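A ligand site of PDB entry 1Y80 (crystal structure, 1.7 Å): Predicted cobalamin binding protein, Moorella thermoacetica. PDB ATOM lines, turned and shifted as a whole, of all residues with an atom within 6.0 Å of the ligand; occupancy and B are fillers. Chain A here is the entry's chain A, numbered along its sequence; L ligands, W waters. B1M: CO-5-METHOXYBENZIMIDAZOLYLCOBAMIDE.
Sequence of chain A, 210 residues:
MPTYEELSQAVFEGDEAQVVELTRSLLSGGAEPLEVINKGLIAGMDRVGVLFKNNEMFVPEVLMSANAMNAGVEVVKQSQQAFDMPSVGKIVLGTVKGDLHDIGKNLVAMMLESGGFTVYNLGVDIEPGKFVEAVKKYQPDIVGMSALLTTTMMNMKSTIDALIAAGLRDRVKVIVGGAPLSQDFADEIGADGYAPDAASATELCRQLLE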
ATOM      1  N   LEU A  93      22.593  -4.026 -29.160  1.00  0.00           N
ATOM      2  CA  LEU A  93      22.285  -2.843 -28.336  1.00  0.00           C
ATOM      3  C   LEU A  93      22.149  -1.590 -29.195  1.00  0.00           C
ATOM      4  O   LEU A  93      22.928  -1.389 -30.124  1.00  0.00           O
ATOM      5  CB  LEU A  93      23.394  -2.569 -27.308  1.00  0.00           C
ATOM      6  CG  LEU A  93      23.596  -3.523 -26.143  1.00  0.00           C
ATOM      7  CD1 LEU A  93      24.695  -2.951 -25.231  1.00  0.00           C
ATOM      8  CD2 LEU A  93      22.305  -3.731 -25.371  1.00  0.00           C
ATOM      9  N   GLY A  98      15.165   8.850 -32.412  1.00  0.00           N
ATOM     10  CA  GLY A  98      14.981  10.188 -31.866  1.00  0.00           C
ATOM     11  C   GLY A  98      15.954  10.561 -30.757  1.00  0.00           C
ATOM     12  O   GLY A  98      15.994  11.720 -30.326  1.00  0.00           O
ATOM     13  N   ASP A  99      16.734   9.579 -30.317  1.00  0.00           N
ATOM     14  CA  ASP A  99      17.571   9.705 -29.122  1.00  0.00           C
ATOM     15  C   ASP A  99      19.063   9.588 -29.498  1.00  0.00           C
ATOM     16  O   ASP A  99      19.441   8.672 -30.192  1.00  0.00           O
ATOM     17  CB  ASP A  99      17.166   8.654 -28.087  1.00  0.00           C
ATOM     18  CG  ASP A  99      17.518   9.042 -26.654  1.00  0.00           C
ATOM     19  OD1 ASP A  99      18.602   9.598 -26.450  1.00  0.00           O
ATOM     20  OD2 ASP A  99      16.677   8.808 -25.742  1.00  0.00           O
ATOM     21  N   LEU A 100      19.887  10.526 -29.032  1.00  0.00           N
ATOM     22  CA  LEU A 100      21.298  10.590 -29.388  1.00  0.00           C
ATOM     23  C   LEU A 100      22.214  10.326 -28.180  1.00  0.00           C
ATOM     24  O   LEU A 100      23.437  10.416 -28.288  1.00  0.00           O
ATOM     25  CB  LEU A 100      21.627  11.941 -30.012  1.00  0.00           C
ATOM     26  CG  LEU A 100      20.796  12.341 -31.233  1.00  0.00           C
ATOM     27  CD1 LEU A 100      21.207  13.722 -31.752  1.00  0.00           C
ATOM     28  CD2 LEU A 100      20.940  11.281 -32.330  1.00  0.00           C
ATOM     29  N   HIS A 101      21.620   9.981 -27.028  1.00  0.00           N
ATOM     30  CA  HIS A 101      22.387   9.697 -25.794  1.00  0.00           C
ATOM     31  C   HIS A 101      22.961   8.283 -25.874  1.00  0.00           C
ATOM     32  O   HIS A 101      22.216   7.343 -26.106  1.00  0.00           O
ATOM     33  CB  HIS A 101      21.492   9.823 -24.549  1.00  0.00           C
ATOM     34  CG  HIS A 101      20.897  11.196 -24.344  1.00  0.00           C
ATOM     35  ND1 HIS A 101      19.760  11.636 -24.998  1.00  0.00           N
ATOM     36  CD2 HIS A 101      21.288  12.223 -23.546  1.00  0.00           C
ATOM     37  CE1 HIS A 101      19.486  12.869 -24.619  1.00  0.00           C
ATOM     38  NE2 HIS A 101      20.396  13.262 -23.744  1.00  0.00           N
ATOM     39  N   ASP A 102      24.272   8.138 -25.640  1.00  0.00           N
ATOM     40  CA  ASP A 102      24.899   6.793 -25.662  1.00  0.00           C
ATOM     41  C   ASP A 102      25.986   6.522 -24.607  1.00  0.00           C
ATOM     42  O   ASP A 102      26.559   5.437 -24.584  1.00  0.00           O
ATOM     43  CB  ASP A 102      25.445   6.489 -27.059  1.00  0.00           C
ATOM     44  CG  ASP A 102      26.569   7.408 -27.484  1.00  0.00           C
ATOM     45  OD1 ASP A 102      27.089   8.173 -26.643  1.00  0.00           O
ATOM     46  OD2 ASP A 102      26.921   7.372 -28.690  1.00  0.00           O
ATOM     47  N   ILE A 103      26.252   7.483 -23.720  1.00  0.00           N
ATOM     48  CA  ILE A 103      27.247   7.283 -22.648  1.00  0.00           C
ATOM     49  C   ILE A 103      26.866   6.072 -21.754  1.00  0.00           C
ATOM     50  O   ILE A 103      27.706   5.195 -21.500  1.00  0.00           O
ATOM     51  CB  ILE A 103      27.436   8.586 -21.807  1.00  0.00           C
ATOM     52  CG1 ILE A 103      28.132   9.655 -22.648  1.00  0.00           C
ATOM     53  CG2 ILE A 103      28.257   8.322 -20.525  1.00  0.00           C
ATOM     54  CD1 ILE A 103      28.035  11.086 -22.050  1.00  0.00           C
ATOM     55  N   GLY A 104      25.602   6.029 -21.302  1.00  0.00           N
ATOM     56  CA  GLY A 104      25.101   4.942 -20.490  1.00  0.00           C
ATOM     57  C   GLY A 104      25.125   3.618 -21.237  1.00  0.00           C
ATOM     58  O   GLY A 104      25.637   2.612 -20.735  1.00  0.00           O
ATOM     59  N   LYS A 105      24.553   3.613 -22.451  1.00  0.00           N
ATOM     60  CA  LYS A 105      24.541   2.425 -23.312  1.00  0.00           C
ATOM     61  C   LYS A 105      25.955   1.868 -23.509  1.00  0.00           C
ATOM     62  O   LYS A 105      26.177   0.646 -23.444  1.00  0.00           O
ATOM     63  CB  LYS A 105      23.934   2.782 -24.690  1.00  0.00           C
ATOM     64  CG  LYS A 105      24.063   1.654 -25.764  1.00  0.00           C
ATOM     65  CD  LYS A 105      23.425   2.029 -27.088  1.00  0.00           C
ATOM     66  CE  LYS A 105      24.090   3.226 -27.804  1.00  0.00           C
ATOM     67  NZ  LYS A 105      25.527   3.025 -28.095  1.00  0.00           N
ATOM     68  N   LEU A 107      28.594   2.228 -21.544  1.00  0.00           N
ATOM     69  CA  LEU A 107      29.057   1.598 -20.290  1.00  0.00           C
ATOM     70  C   LEU A 107      28.438   0.203 -20.107  1.00  0.00           C
ATOM     71  O   LEU A 107      29.125  -0.748 -19.720  1.00  0.00           O
ATOM     72  CB  LEU A 107      28.736   2.496 -19.082  1.00  0.00           C
ATOM     73  CG  LEU A 107      29.240   1.996 -17.718  1.00  0.00           C
ATOM     74  CD1 LEU A 107      30.718   1.675 -17.769  1.00  0.00           C
ATOM     75  CD2 LEU A 107      28.966   3.028 -16.605  1.00  0.00           C
ATOM     76  N   VAL A 108      27.137   0.072 -20.403  1.00  0.00           N
ATOM     77  CA  VAL A 108      26.470  -1.215 -20.396  1.00  0.00           C
ATOM     78  C   VAL A 108      27.203  -2.200 -21.338  1.00  0.00           C
ATOM     79  O   VAL A 108      27.492  -3.329 -20.960  1.00  0.00           O
ATOM     80  CB  VAL A 108      24.952  -1.074 -20.791  1.00  0.00           C
ATOM     81  CG1 VAL A 108      24.308  -2.442 -20.986  1.00  0.00           C
ATOM     82  CG2 VAL A 108      24.197  -0.234 -19.719  1.00  0.00           C
ATOM     83  N   VAL A 143      18.066  -8.354 -27.336  1.00  0.00           N
ATOM     84  CA  VAL A 143      18.034  -6.993 -27.884  1.00  0.00           C
ATOM     85  C   VAL A 143      17.867  -6.015 -26.733  1.00  0.00           C
ATOM     86  O   VAL A 143      16.939  -6.140 -25.946  1.00  0.00           O
ATOM     87  CB  VAL A 143      16.871  -6.785 -28.895  1.00  0.00           C
ATOM     88  CG1 VAL A 143      16.786  -5.310 -29.330  1.00  0.00           C
ATOM     89  CG2 VAL A 143      17.030  -7.677 -30.086  1.00  0.00           C
ATOM     90  N   GLY A 144      18.795  -5.054 -26.623  1.00  0.00           N
ATOM     91  CA  GLY A 144      18.747  -4.042 -25.578  1.00  0.00           C
ATOM     92  C   GLY A 144      18.541  -2.672 -26.176  1.00  0.00           C
ATOM     93  O   GLY A 144      19.169  -2.314 -27.184  1.00  0.00           O
ATOM     94  N   MET A 145      17.682  -1.896 -25.537  1.00  0.00           N
ATOM     95  CA  MET A 145      17.362  -0.547 -25.969  1.00  0.00           C
ATOM     96  C   MET A 145      17.583   0.446 -24.831  1.00  0.00           C
ATOM     97  O   MET A 145      17.205   0.183 -23.680  1.00  0.00           O
ATOM     98  CB  MET A 145      15.908  -0.490 -26.415  1.00  0.00           C
ATOM     99  CG  MET A 145      15.640  -1.303 -27.663  1.00  0.00           C
ATOM    100  SD  MET A 145      13.951  -1.051 -28.268  1.00  0.00           S
ATOM    101  CE  MET A 145      13.050  -2.150 -27.216  1.00  0.00           C
ATOM    102  N   SER A 146      18.201   1.576 -25.158  1.00  0.00           N
ATOM    103  CA  SER A 146      18.429   2.643 -24.224  1.00  0.00           C
ATOM    104  C   SER A 146      17.662   3.862 -24.667  1.00  0.00           C
ATOM    105  O   SER A 146      17.574   4.140 -25.848  1.00  0.00           O
ATOM    106  CB  SER A 146      19.944   2.960 -24.136  1.00  0.00           C
ATOM    107  OG  SER A 146      20.233   3.926 -23.144  1.00  0.00           O
ATOM    108  N   ALA A 147      17.072   4.580 -23.704  1.00  0.00           N
ATOM    109  CA  ALA A 147      16.448   5.881 -23.976  1.00  0.00           C
ATOM    110  C   ALA A 147      16.671   6.781 -22.783  1.00  0.00           C
ATOM    111  O   ALA A 147      16.506   6.338 -21.621  1.00  0.00           O
ATOM    112  CB  ALA A 147      14.987   5.727 -24.242  1.00  0.00           C
ATOM    113  N   LEU A 148      17.072   8.016 -23.040  1.00  0.00           N
ATOM    114  CA  LEU A 148      17.225   9.027 -21.988  1.00  0.00           C
ATOM    115  C   LEU A 148      16.176  10.120 -22.047  1.00  0.00           C
ATOM    116  O   LEU A 148      16.014  10.861 -21.064  1.00  0.00           O
ATOM    117  CB  LEU A 148      18.634   9.656 -21.993  1.00  0.00           C
ATOM    118  CG  LEU A 148      19.794   8.942 -21.292  1.00  0.00           C
ATOM    119  CD1 LEU A 148      19.696   9.128 -19.812  1.00  0.00           C
ATOM    120  CD2 LEU A 148      19.887   7.445 -21.668  1.00  0.00           C
ATOM    121  N   LEU A 149      15.482  10.246 -23.175  1.00  0.00           N
ATOM    122  CA  LEU A 149      14.384  11.210 -23.332  1.00  0.00           C
ATOM    123  C   LEU A 149      13.042  10.537 -23.038  1.00  0.00           C
ATOM    124  O   LEU A 149      12.732   9.494 -23.608  1.00  0.00           O
ATOM    125  CB  LEU A 149      14.353  11.756 -24.752  1.00  0.00           C
ATOM    126  CG  LEU A 149      15.599  12.479 -25.254  1.00  0.00           C
ATOM    127  CD1 LEU A 149      15.474  12.795 -26.772  1.00  0.00           C
ATOM    128  CD2 LEU A 149      15.826  13.744 -24.436  1.00  0.00           C
ATOM    129  N   THR A 150      12.252  11.119 -22.141  1.00  0.00           N
ATOM    130  CA  THR A 150      10.857  10.669 -21.931  1.00  0.00           C
ATOM    131  C   THR A 150      10.094  10.545 -23.265  1.00  0.00           C
ATOM    132  O   THR A 150       9.301   9.638 -23.448  1.00  0.00           O
ATOM    133  CB  THR A 150      10.098  11.616 -20.966  1.00  0.00           C
ATOM    134  OG1 THR A 150      10.039  12.919 -21.516  1.00  0.00           O
ATOM    135  CG2 THR A 150      10.783  11.705 -19.635  1.00  0.00           C
ATOM    136  N   THR A 151      10.379  11.454 -24.199  1.00  0.00           N
ATOM    137  CA  THR A 151       9.685  11.520 -25.479  1.00  0.00           C
ATOM    138  C   THR A 151      10.154  10.477 -26.512  1.00  0.00           C
ATOM    139  O   THR A 151       9.563  10.369 -27.583  1.00  0.00           O
ATOM    140  CB  THR A 151       9.839  12.912 -26.100  1.00  0.00           C
ATOM    141  OG1 THR A 151      11.233  13.298 -26.145  1.00  0.00           O
ATOM    142  CG2 THR A 151       9.060  13.926 -25.297  1.00  0.00           C
ATOM    143  N   ILE A 175      15.462  -6.209 -23.476  1.00  0.00           N
ATOM    144  CA  ILE A 175      15.745  -5.485 -22.234  1.00  0.00           C
ATOM    145  C   ILE A 175      15.765  -3.977 -22.524  1.00  0.00           C
ATOM    146  O   ILE A 175      16.156  -3.561 -23.593  1.00  0.00           O
ATOM    147  CB  ILE A 175      17.015  -5.969 -21.517  1.00  0.00           C
ATOM    148  CG1 ILE A 175      18.266  -5.787 -22.369  1.00  0.00           C
ATOM    149  CG2 ILE A 175      16.855  -7.422 -21.135  1.00  0.00           C
ATOM    150  CD1 ILE A 175      19.534  -5.860 -21.577  1.00  0.00           C
ATOM    151  N   VAL A 176      15.316  -3.187 -21.567  1.00  0.00           N
ATOM    152  CA  VAL A 176      15.294  -1.730 -21.702  1.00  0.00           C
ATOM    153  C   VAL A 176      15.971  -1.063 -20.485  1.00  0.00           C
ATOM    154  O   VAL A 176      15.955  -1.610 -19.370  1.00  0.00           O
ATOM    155  CB  VAL A 176      13.843  -1.207 -21.909  1.00  0.00           C
ATOM    156  CG1 VAL A 176      13.233  -1.884 -23.167  1.00  0.00           C
ATOM    157  CG2 VAL A 176      12.963  -1.461 -20.644  1.00  0.00           C
ATOM    158  N   GLY A 177      16.589   0.087 -20.732  1.00  0.00           N
ATOM    159  CA  GLY A 177      17.182   0.887 -19.675  1.00  0.00           C
ATOM    160  C   GLY A 177      17.328   2.341 -20.066  1.00  0.00           C
ATOM    161  O   GLY A 177      16.992   2.761 -21.200  1.00  0.00           O
ATOM    162  N   GLY A 178      17.860   3.121 -19.110  1.00  0.00           N
ATOM    163  CA  GLY A 178      17.950   4.551 -19.232  1.00  0.00           C
ATOM    164  C   GLY A 178      17.398   5.181 -17.976  1.00  0.00           C
ATOM    165  O   GLY A 178      16.534   4.606 -17.315  1.00  0.00           O
ATOM    166  N   ALA A 179      17.897   6.370 -17.658  1.00  0.00           N
ATOM    167  CA  ALA A 179      17.426   7.122 -16.476  1.00  0.00           C
ATOM    168  C   ALA A 179      15.877   7.174 -16.294  1.00  0.00           C
ATOM    169  O   ALA A 179      15.400   6.965 -15.161  1.00  0.00           O
ATOM    170  CB  ALA A 179      18.019   8.523 -16.467  1.00  0.00           C
ATOM    171  N   PRO A 180      15.100   7.477 -17.379  1.00  0.00           N
ATOM    172  CA  PRO A 180      13.624   7.534 -17.203  1.00  0.00           C
ATOM    173  C   PRO A 180      12.909   6.174 -17.209  1.00  0.00           C
ATOM    174  O   PRO A 180      11.695   6.094 -16.939  1.00  0.00           O
ATOM    175  CB  PRO A 180      13.164   8.381 -18.381  1.00  0.00           C
ATOM    176  CG  PRO A 180      14.182   8.158 -19.446  1.00  0.00           C
ATOM    177  CD  PRO A 180      15.498   7.806 -18.767  1.00  0.00           C
ATOM    178  N   ALA A 195      16.833  -3.009 -16.214  1.00  0.00           N
ATOM    179  CA  ALA A 195      17.907  -2.918 -15.227  1.00  0.00           C
ATOM    180  C   ALA A 195      18.206  -1.436 -14.975  1.00  0.00           C
ATOM    181  O   ALA A 195      18.235  -0.646 -15.928  1.00  0.00           O
ATOM    182  CB  ALA A 195      19.139  -3.635 -15.718  1.00  0.00           C
ATOM    183  N   PRO A 196      18.407  -1.046 -13.694  1.00  0.00           N
ATOM    184  CA  PRO A 196      18.681   0.351 -13.364  1.00  0.00           C
ATOM    185  C   PRO A 196      20.073   0.838 -13.714  1.00  0.00           C
ATOM    186  O   PRO A 196      20.295   2.030 -13.793  1.00  0.00           O
ATOM    187  CB  PRO A 196      18.482   0.383 -11.836  1.00  0.00           C
ATOM    188  CG  PRO A 196      18.861  -1.007 -11.397  1.00  0.00           C
ATOM    189  CD  PRO A 196      18.321  -1.897 -12.477  1.00  0.00           C
ATOM    190  N   ASP A 197      21.027  -0.065 -13.895  1.00  0.00           N
ATOM    191  CA  ASP A 197      22.420   0.342 -14.152  1.00  0.00           C
ATOM    192  C   ASP A 197      23.196  -0.744 -14.897  1.00  0.00           C
ATOM    193  O   ASP A 197      22.657  -1.831 -15.144  1.00  0.00           O
ATOM    194  CB  ASP A 197      23.137   0.760 -12.847  1.00  0.00           C
ATOM    195  CG  ASP A 197      23.107  -0.334 -11.751  1.00  0.00           C
ATOM    196  OD1 ASP A 197      23.222  -1.539 -12.056  1.00  0.00           O
ATOM    197  OD2 ASP A 197      23.006   0.052 -10.556  1.00  0.00           O
ATOM    198  N   ALA A 198      24.438  -0.451 -15.250  1.00  0.00           N
ATOM    199  CA  ALA A 198      25.236  -1.373 -16.044  1.00  0.00           C
ATOM    200  C   ALA A 198      25.499  -2.712 -15.314  1.00  0.00           C
ATOM    201  O   ALA A 198      25.348  -3.782 -15.924  1.00  0.00           O
ATOM    202  CB  ALA A 198      26.512  -0.749 -16.448  1.00  0.00           C
ATOM    203  N   ALA A 199      25.886  -2.648 -14.037  1.00  0.00           N
ATOM    204  CA  ALA A 199      26.173  -3.882 -13.272  1.00  0.00           C
ATOM    205  C   ALA A 199      24.938  -4.792 -13.234  1.00  0.00           C
ATOM    206  O   ALA A 199      25.033  -5.990 -13.527  1.00  0.00           O
ATOM    207  CB  ALA A 199      26.632  -3.550 -11.866  1.00  0.00           C
ATOM    208  N   ALA A 201      22.373  -4.698 -15.248  1.00  0.00           N
ATOM    209  CA  ALA A 201      22.070  -5.095 -16.641  1.00  0.00           C
ATOM    210  C   ALA A 201      22.815  -6.386 -17.014  1.00  0.00           C
ATOM    211  O   ALA A 201      22.261  -7.252 -17.689  1.00  0.00           O
ATOM    212  CB  ALA A 201      22.419  -3.994 -17.600  1.00  0.00           C
HETATM  213 CO   B1M L   1      20.675  15.506 -22.884  1.00  0.00          CO
HETATM  214  N21 B1M L   1      19.174  15.484 -21.812  1.00  0.00           N
HETATM  215  N22 B1M L   1      19.706  16.312 -24.305  1.00  0.00           N
HETATM  216  N23 B1M L   1      22.289  15.439 -23.834  1.00  0.00           N
HETATM  217  N24 B1M L   1      21.507  14.988 -21.282  1.00  0.00           N
HETATM  218  C1  B1M L   1      19.283  14.828 -20.523  1.00  0.00           C
HETATM  219  C20 B1M L   1      19.044  13.344 -20.729  1.00  0.00           C
HETATM  220  C2  B1M L   1      18.216  15.569 -19.649  1.00  0.00           C
HETATM  221  C25 B1M L   1      17.657  14.734 -18.484  1.00  0.00           C
HETATM  222  C26 B1M L   1      18.709  16.961 -19.133  1.00  0.00           C
HETATM  223  C27 B1M L   1      17.707  17.627 -18.168  1.00  0.00           C
HETATM  224  O28 B1M L   1      17.926  17.658 -16.967  1.00  0.00           O
HETATM  225  N29 B1M L   1      16.599  18.173 -18.642  1.00  0.00           N
HETATM  226  C3  B1M L   1      17.169  15.874 -20.750  1.00  0.00           C
HETATM  227  C30 B1M L   1      16.029  14.868 -20.977  1.00  0.00           C
HETATM  228  C31 B1M L   1      14.839  15.149 -20.074  1.00  0.00           C
HETATM  229  C32 B1M L   1      13.809  14.065 -20.207  1.00  0.00           C
HETATM  230  O34 B1M L   1      13.490  13.371 -19.245  1.00  0.00           O
HETATM  231  N33 B1M L   1      13.300  13.941 -21.409  1.00  0.00           N
HETATM  232  C4  B1M L   1      18.037  16.032 -21.979  1.00  0.00           C
HETATM  233  C5  B1M L   1      17.641  16.763 -23.170  1.00  0.00           C
HETATM  234  C35 B1M L   1      16.246  17.401 -23.172  1.00  0.00           C
HETATM  235  C6  B1M L   1      18.469  16.875 -24.234  1.00  0.00           C
HETATM  236  C7  B1M L   1      18.187  17.715 -25.510  1.00  0.00           C
HETATM  237  C36 B1M L   1      16.745  17.725 -26.059  1.00  0.00           C
HETATM  238  C37 B1M L   1      18.663  19.163 -25.186  1.00  0.00           C
HETATM  239  C38 B1M L   1      18.432  20.141 -26.346  1.00  0.00           C
HETATM  240  O39 B1M L   1      17.375  20.697 -26.464  1.00  0.00           O
HETATM  241  N40 B1M L   1      19.431  20.333 -27.188  1.00  0.00           N
HETATM  242  C8  B1M L   1      19.151  17.017 -26.452  1.00  0.00           C
HETATM  243  C41 B1M L   1      18.524  15.864 -27.246  1.00  0.00           C
HETATM  244  C42 B1M L   1      19.434  15.147 -28.237  1.00  0.00           C
HETATM  245  C43 B1M L   1      18.635  13.938 -28.713  1.00  0.00           C
HETATM  246  O44 B1M L   1      17.970  13.943 -29.768  1.00  0.00           O
HETATM  247  N45 B1M L   1      18.671  12.890 -27.932  1.00  0.00           N
HETATM  248  C9  B1M L   1      20.155  16.490 -25.485  1.00  0.00           C
HETATM  249  C10 B1M L   1      21.527  16.293 -25.901  1.00  0.00           C
HETATM  250  C11 B1M L   1      22.472  15.830 -25.120  1.00  0.00           C
HETATM  251  C12 B1M L   1      23.890  15.611 -25.613  1.00  0.00           C
HETATM  252  C46 B1M L   1      23.894  15.032 -27.046  1.00  0.00           C
HETATM  253  C47 B1M L   1      24.613  16.923 -25.564  1.00  0.00           C
HETATM  254  C13 B1M L   1      24.437  14.713 -24.518  1.00  0.00           C
HETATM  255  C48 B1M L   1      24.625  13.221 -24.869  1.00  0.00           C
HETATM  256  C49 B1M L   1      26.061  12.924 -25.316  1.00  0.00           C
HETATM  257  C50 B1M L   1      26.150  11.452 -25.681  1.00  0.00           C
HETATM  258  O51 B1M L   1      25.639  10.598 -24.977  1.00  0.00           O
HETATM  259  N52 B1M L   1      26.806  11.180 -26.822  1.00  0.00           N
HETATM  260  C14 B1M L   1      23.414  14.893 -23.408  1.00  0.00           C
HETATM  261  C15 B1M L   1      23.717  14.482 -22.036  1.00  0.00           C
HETATM  262  C53 B1M L   1      25.106  13.880 -21.725  1.00  0.00           C
HETATM  263  C16 B1M L   1      22.784  14.633 -21.043  1.00  0.00           C
HETATM  264  C17 B1M L   1      23.023  14.500 -19.510  1.00  0.00           C
HETATM  265  C54 B1M L   1      23.768  15.776 -19.100  1.00  0.00           C
HETATM  266  C55 B1M L   1      23.779  13.227 -19.018  1.00  0.00           C
HETATM  267  C56 B1M L   1      23.306  11.861 -19.550  1.00  0.00           C
HETATM  268  C57 B1M L   1      24.355  10.816 -19.188  1.00  0.00           C
HETATM  269  O58 B1M L   1      25.219  10.540 -20.008  1.00  0.00           O
HETATM  270  N59 B1M L   1      24.297  10.320 -17.954  1.00  0.00           N
HETATM  271  C18 B1M L   1      21.558  14.463 -18.966  1.00  0.00           C
HETATM  272  C60 B1M L   1      21.309  15.199 -17.628  1.00  0.00           C
HETATM  273  C61 B1M L   1      22.022  14.483 -16.459  1.00  0.00           C
HETATM  274  O63 B1M L   1      23.061  14.903 -15.958  1.00  0.00           O
HETATM  275  N62 B1M L   1      21.449  13.376 -16.006  1.00  0.00           N
HETATM  276  C19 B1M L   1      20.778  14.871 -20.223  1.00  0.00           C
HETATM  277  C1P B1M L   1      25.320   9.417 -17.407  1.00  0.00           C
HETATM  278  C2P B1M L   1      25.076   7.981 -17.781  1.00  0.00           C
HETATM  279  C3P B1M L   1      26.205   7.089 -17.237  1.00  0.00           C
HETATM  280  O3  B1M L   1      23.820   7.583 -17.207  1.00  0.00           O
HETATM  281  O4  B1M L   1      22.699   7.374 -19.487  1.00  0.00           O
HETATM  282  O5  B1M L   1      21.349   7.141 -17.312  1.00  0.00           O
HETATM  283  P   B1M L   1      22.626   6.924 -18.059  1.00  0.00           P
HETATM  284  O2  B1M L   1      22.945   5.344 -18.068  1.00  0.00           O
HETATM  285  C3R B1M L   1      22.956   4.481 -16.932  1.00  0.00           C
HETATM  286  C2R B1M L   1      21.561   3.953 -16.595  1.00  0.00           C
HETATM  287  O7R B1M L   1      20.476   4.665 -17.175  1.00  0.00           O
HETATM  288  C1R B1M L   1      21.566   2.513 -17.082  1.00  0.00           C
HETATM  289  O6R B1M L   1      22.931   2.124 -16.912  1.00  0.00           O
HETATM  290  C4R B1M L   1      23.757   3.213 -17.281  1.00  0.00           C
HETATM  291  C5R B1M L   1      25.140   3.095 -16.614  1.00  0.00           C
HETATM  292  O8R B1M L   1      25.052   2.590 -15.280  1.00  0.00           O
HETATM  293  N1B B1M L   1      21.226   2.288 -18.527  1.00  0.00           N
HETATM  294  C8B B1M L   1      20.891   1.075 -19.001  1.00  0.00           C
HETATM  295  C2B B1M L   1      21.268   3.151 -19.573  1.00  0.00           C
HETATM  296  N3B B1M L   1      20.926   2.524 -20.738  1.00  0.00           N
HETATM  297  C9B B1M L   1      20.679   1.220 -20.444  1.00  0.00           C
HETATM  298  C4B B1M L   1      20.291   0.099 -21.186  1.00  0.00           C
HETATM  299  C5B B1M L   1      20.137  -1.156 -20.540  1.00  0.00           C
HETATM  300  C6B B1M L   1      20.332  -1.272 -19.153  1.00  0.00           C
HETATM  301  C7B B1M L   1      20.706  -0.165 -18.401  1.00  0.00           C
HETATM  302  O5M B1M L   1      19.768  -2.281 -21.228  1.00  0.00           O
HETATM  303  C5O B1M L   1      19.640  -2.241 -22.649  1.00  0.00           C
HETATM  304  O   HOH W   1      18.484   1.981 -16.669  1.00  0.00           O
HETATM  305  O   HOH W   2      25.331  13.165 -15.479  1.00  0.00           O
HETATM  306  O   HOH W   3      21.080  18.021 -22.154  1.00  0.00           O
HETATM  307  O   HOH W   4      11.664  14.941 -23.457  1.00  0.00           O
HETATM  308  O   HOH W   5      24.323  10.214 -22.512  1.00  0.00           O
HETATM  309  O   HOH W   6      29.299   9.045 -26.007  1.00  0.00           O
HETATM  310  O   HOH W   7      23.388   7.778 -21.966  1.00  0.00           O
HETATM  311  O   HOH W   8      18.569   3.965 -14.469  1.00  0.00           O
HETATM  312  O   HOH W   9      22.305  19.664 -26.578  1.00  0.00           O
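NE2 of His 101 is bound to CO of the ligand, at 2.4 Å. The side-chain hydroxyl (OG) of Ser 146 lies within hydrogen-bond range of a nitrogen (N3B) of the ligand (2.9 Å). The backbone NH (N) of Asp 102 lies within hydrogen-bond range of an oxygen (O51) of the ligand. A nitrogen (N52) of the ligand is in hydrogen-bond range of the side-chain carboxylate (OD1) of Asp 102 (3.0 Å). OG1 of Thr 150 lies within hydrogen-bond range of N33 of the ligand, 3.4 Å away. An oxygen (O8R) of the ligand lies within hydrogen-bond range of the backbone NH (N) of Ala 198, 3.1 Å away. O7R of the ligand is in hydrogen-bond range of N of Ala 179. The backbone NH (N) of Ile 103 lies within hydrogen-bond range of an oxygen (O51) of the ligand, 3.4 Å away.
Water W7 lies within hydrogen-bond range of an oxygen (O4) of the ligand (2.6 Å), the backbone NH of Gly 104 (2.9 Å) and the backbone NH of Ile 103 (3.4 Å). Water W4 lies within hydrogen-bond range of N33 of the ligand, OG1 of Thr 151 and OG1 of Thr 150. Water W1 lies within hydrogen-bond range of the backbone carbonyl oxygen of Ala 195 (2.7 Å), the backbone NH of Gly 178 (2.8 Å), an oxygen (O7R) of the ligand (3.4 Å) and the backbone carbonyl oxygen of Pro 196 (3.4 Å). Water W6 lies within hydrogen-bond range of OD1 of Asp 102 (2.5 Å) and N52 of the ligand (3.4 Å). Water W8 bridges the backbone carbonyl oxygen (O) of Pro 196 and an oxygen (O7R) of the ligand.
The side-chain carboxylate of Asp 99 lies within hydrogen-bond range of a ring nitrogen (ND1) of His 101, at 2.8 Å. The backbone NH (N) of Leu 149 is in hydrogen-bond range of the side-chain carboxylate (OD2) of Asp 99 (3.2 Å). N of Leu 148 sits at hydrogen-bond distance from OD2 of Asp 99 (2.8 Å). O of Met 145 lies within hydrogen-bond range of N of Gly 177 (3.0 Å). N of Met 145 is in hydrogen-bond range of O of Ile 175. O of Gly 177 sits at hydrogen-bond distance from N of Ala 147, 3.1 Å away. O of Val 143 lies within hydrogen-bond range of N of Ile 175 (2.9 Å).
An oxygen (O44) of the ligand lies close to the backbone carbonyl oxygen (O) of Gly 98. N45 of the ligand sits close to N of Leu 100 (2.9 Å). Merely in contact with the ligand: Asp 99 (3.6 Å), Gly 104 (3.3 Å), Leu 107 (3.8 Å), Val 108 (3.6 Å), Gly 144 (3.6 Å), Met 145 (3.5 Å), Leu 148 (3.5 Å), Leu 149 (3.4 Å), Ile 175 (3.6 Å), Gly 177 (3.5 Å), Gly 178 (3.2 Å), Ala 195 (3.5 Å), Pro 196 (3.6 Å), Asp 197 (3.3 Å) and Ala 201 (3.8 Å). 24 residues have an atom within 4 Å of the ligand: Gly 98, Asp 99, Leu 100, His 101, Asp 102, Ile 103, Gly 104, Leu 107, Val 108, Gly 144, Met 145, Ser 146, Leu 148, Leu 149, Thr 150, Ile 175, Gly 177, Gly 178, Ala 179, Ala 195, Pro 196, Asp 197, Ala 198 and Ala 201.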
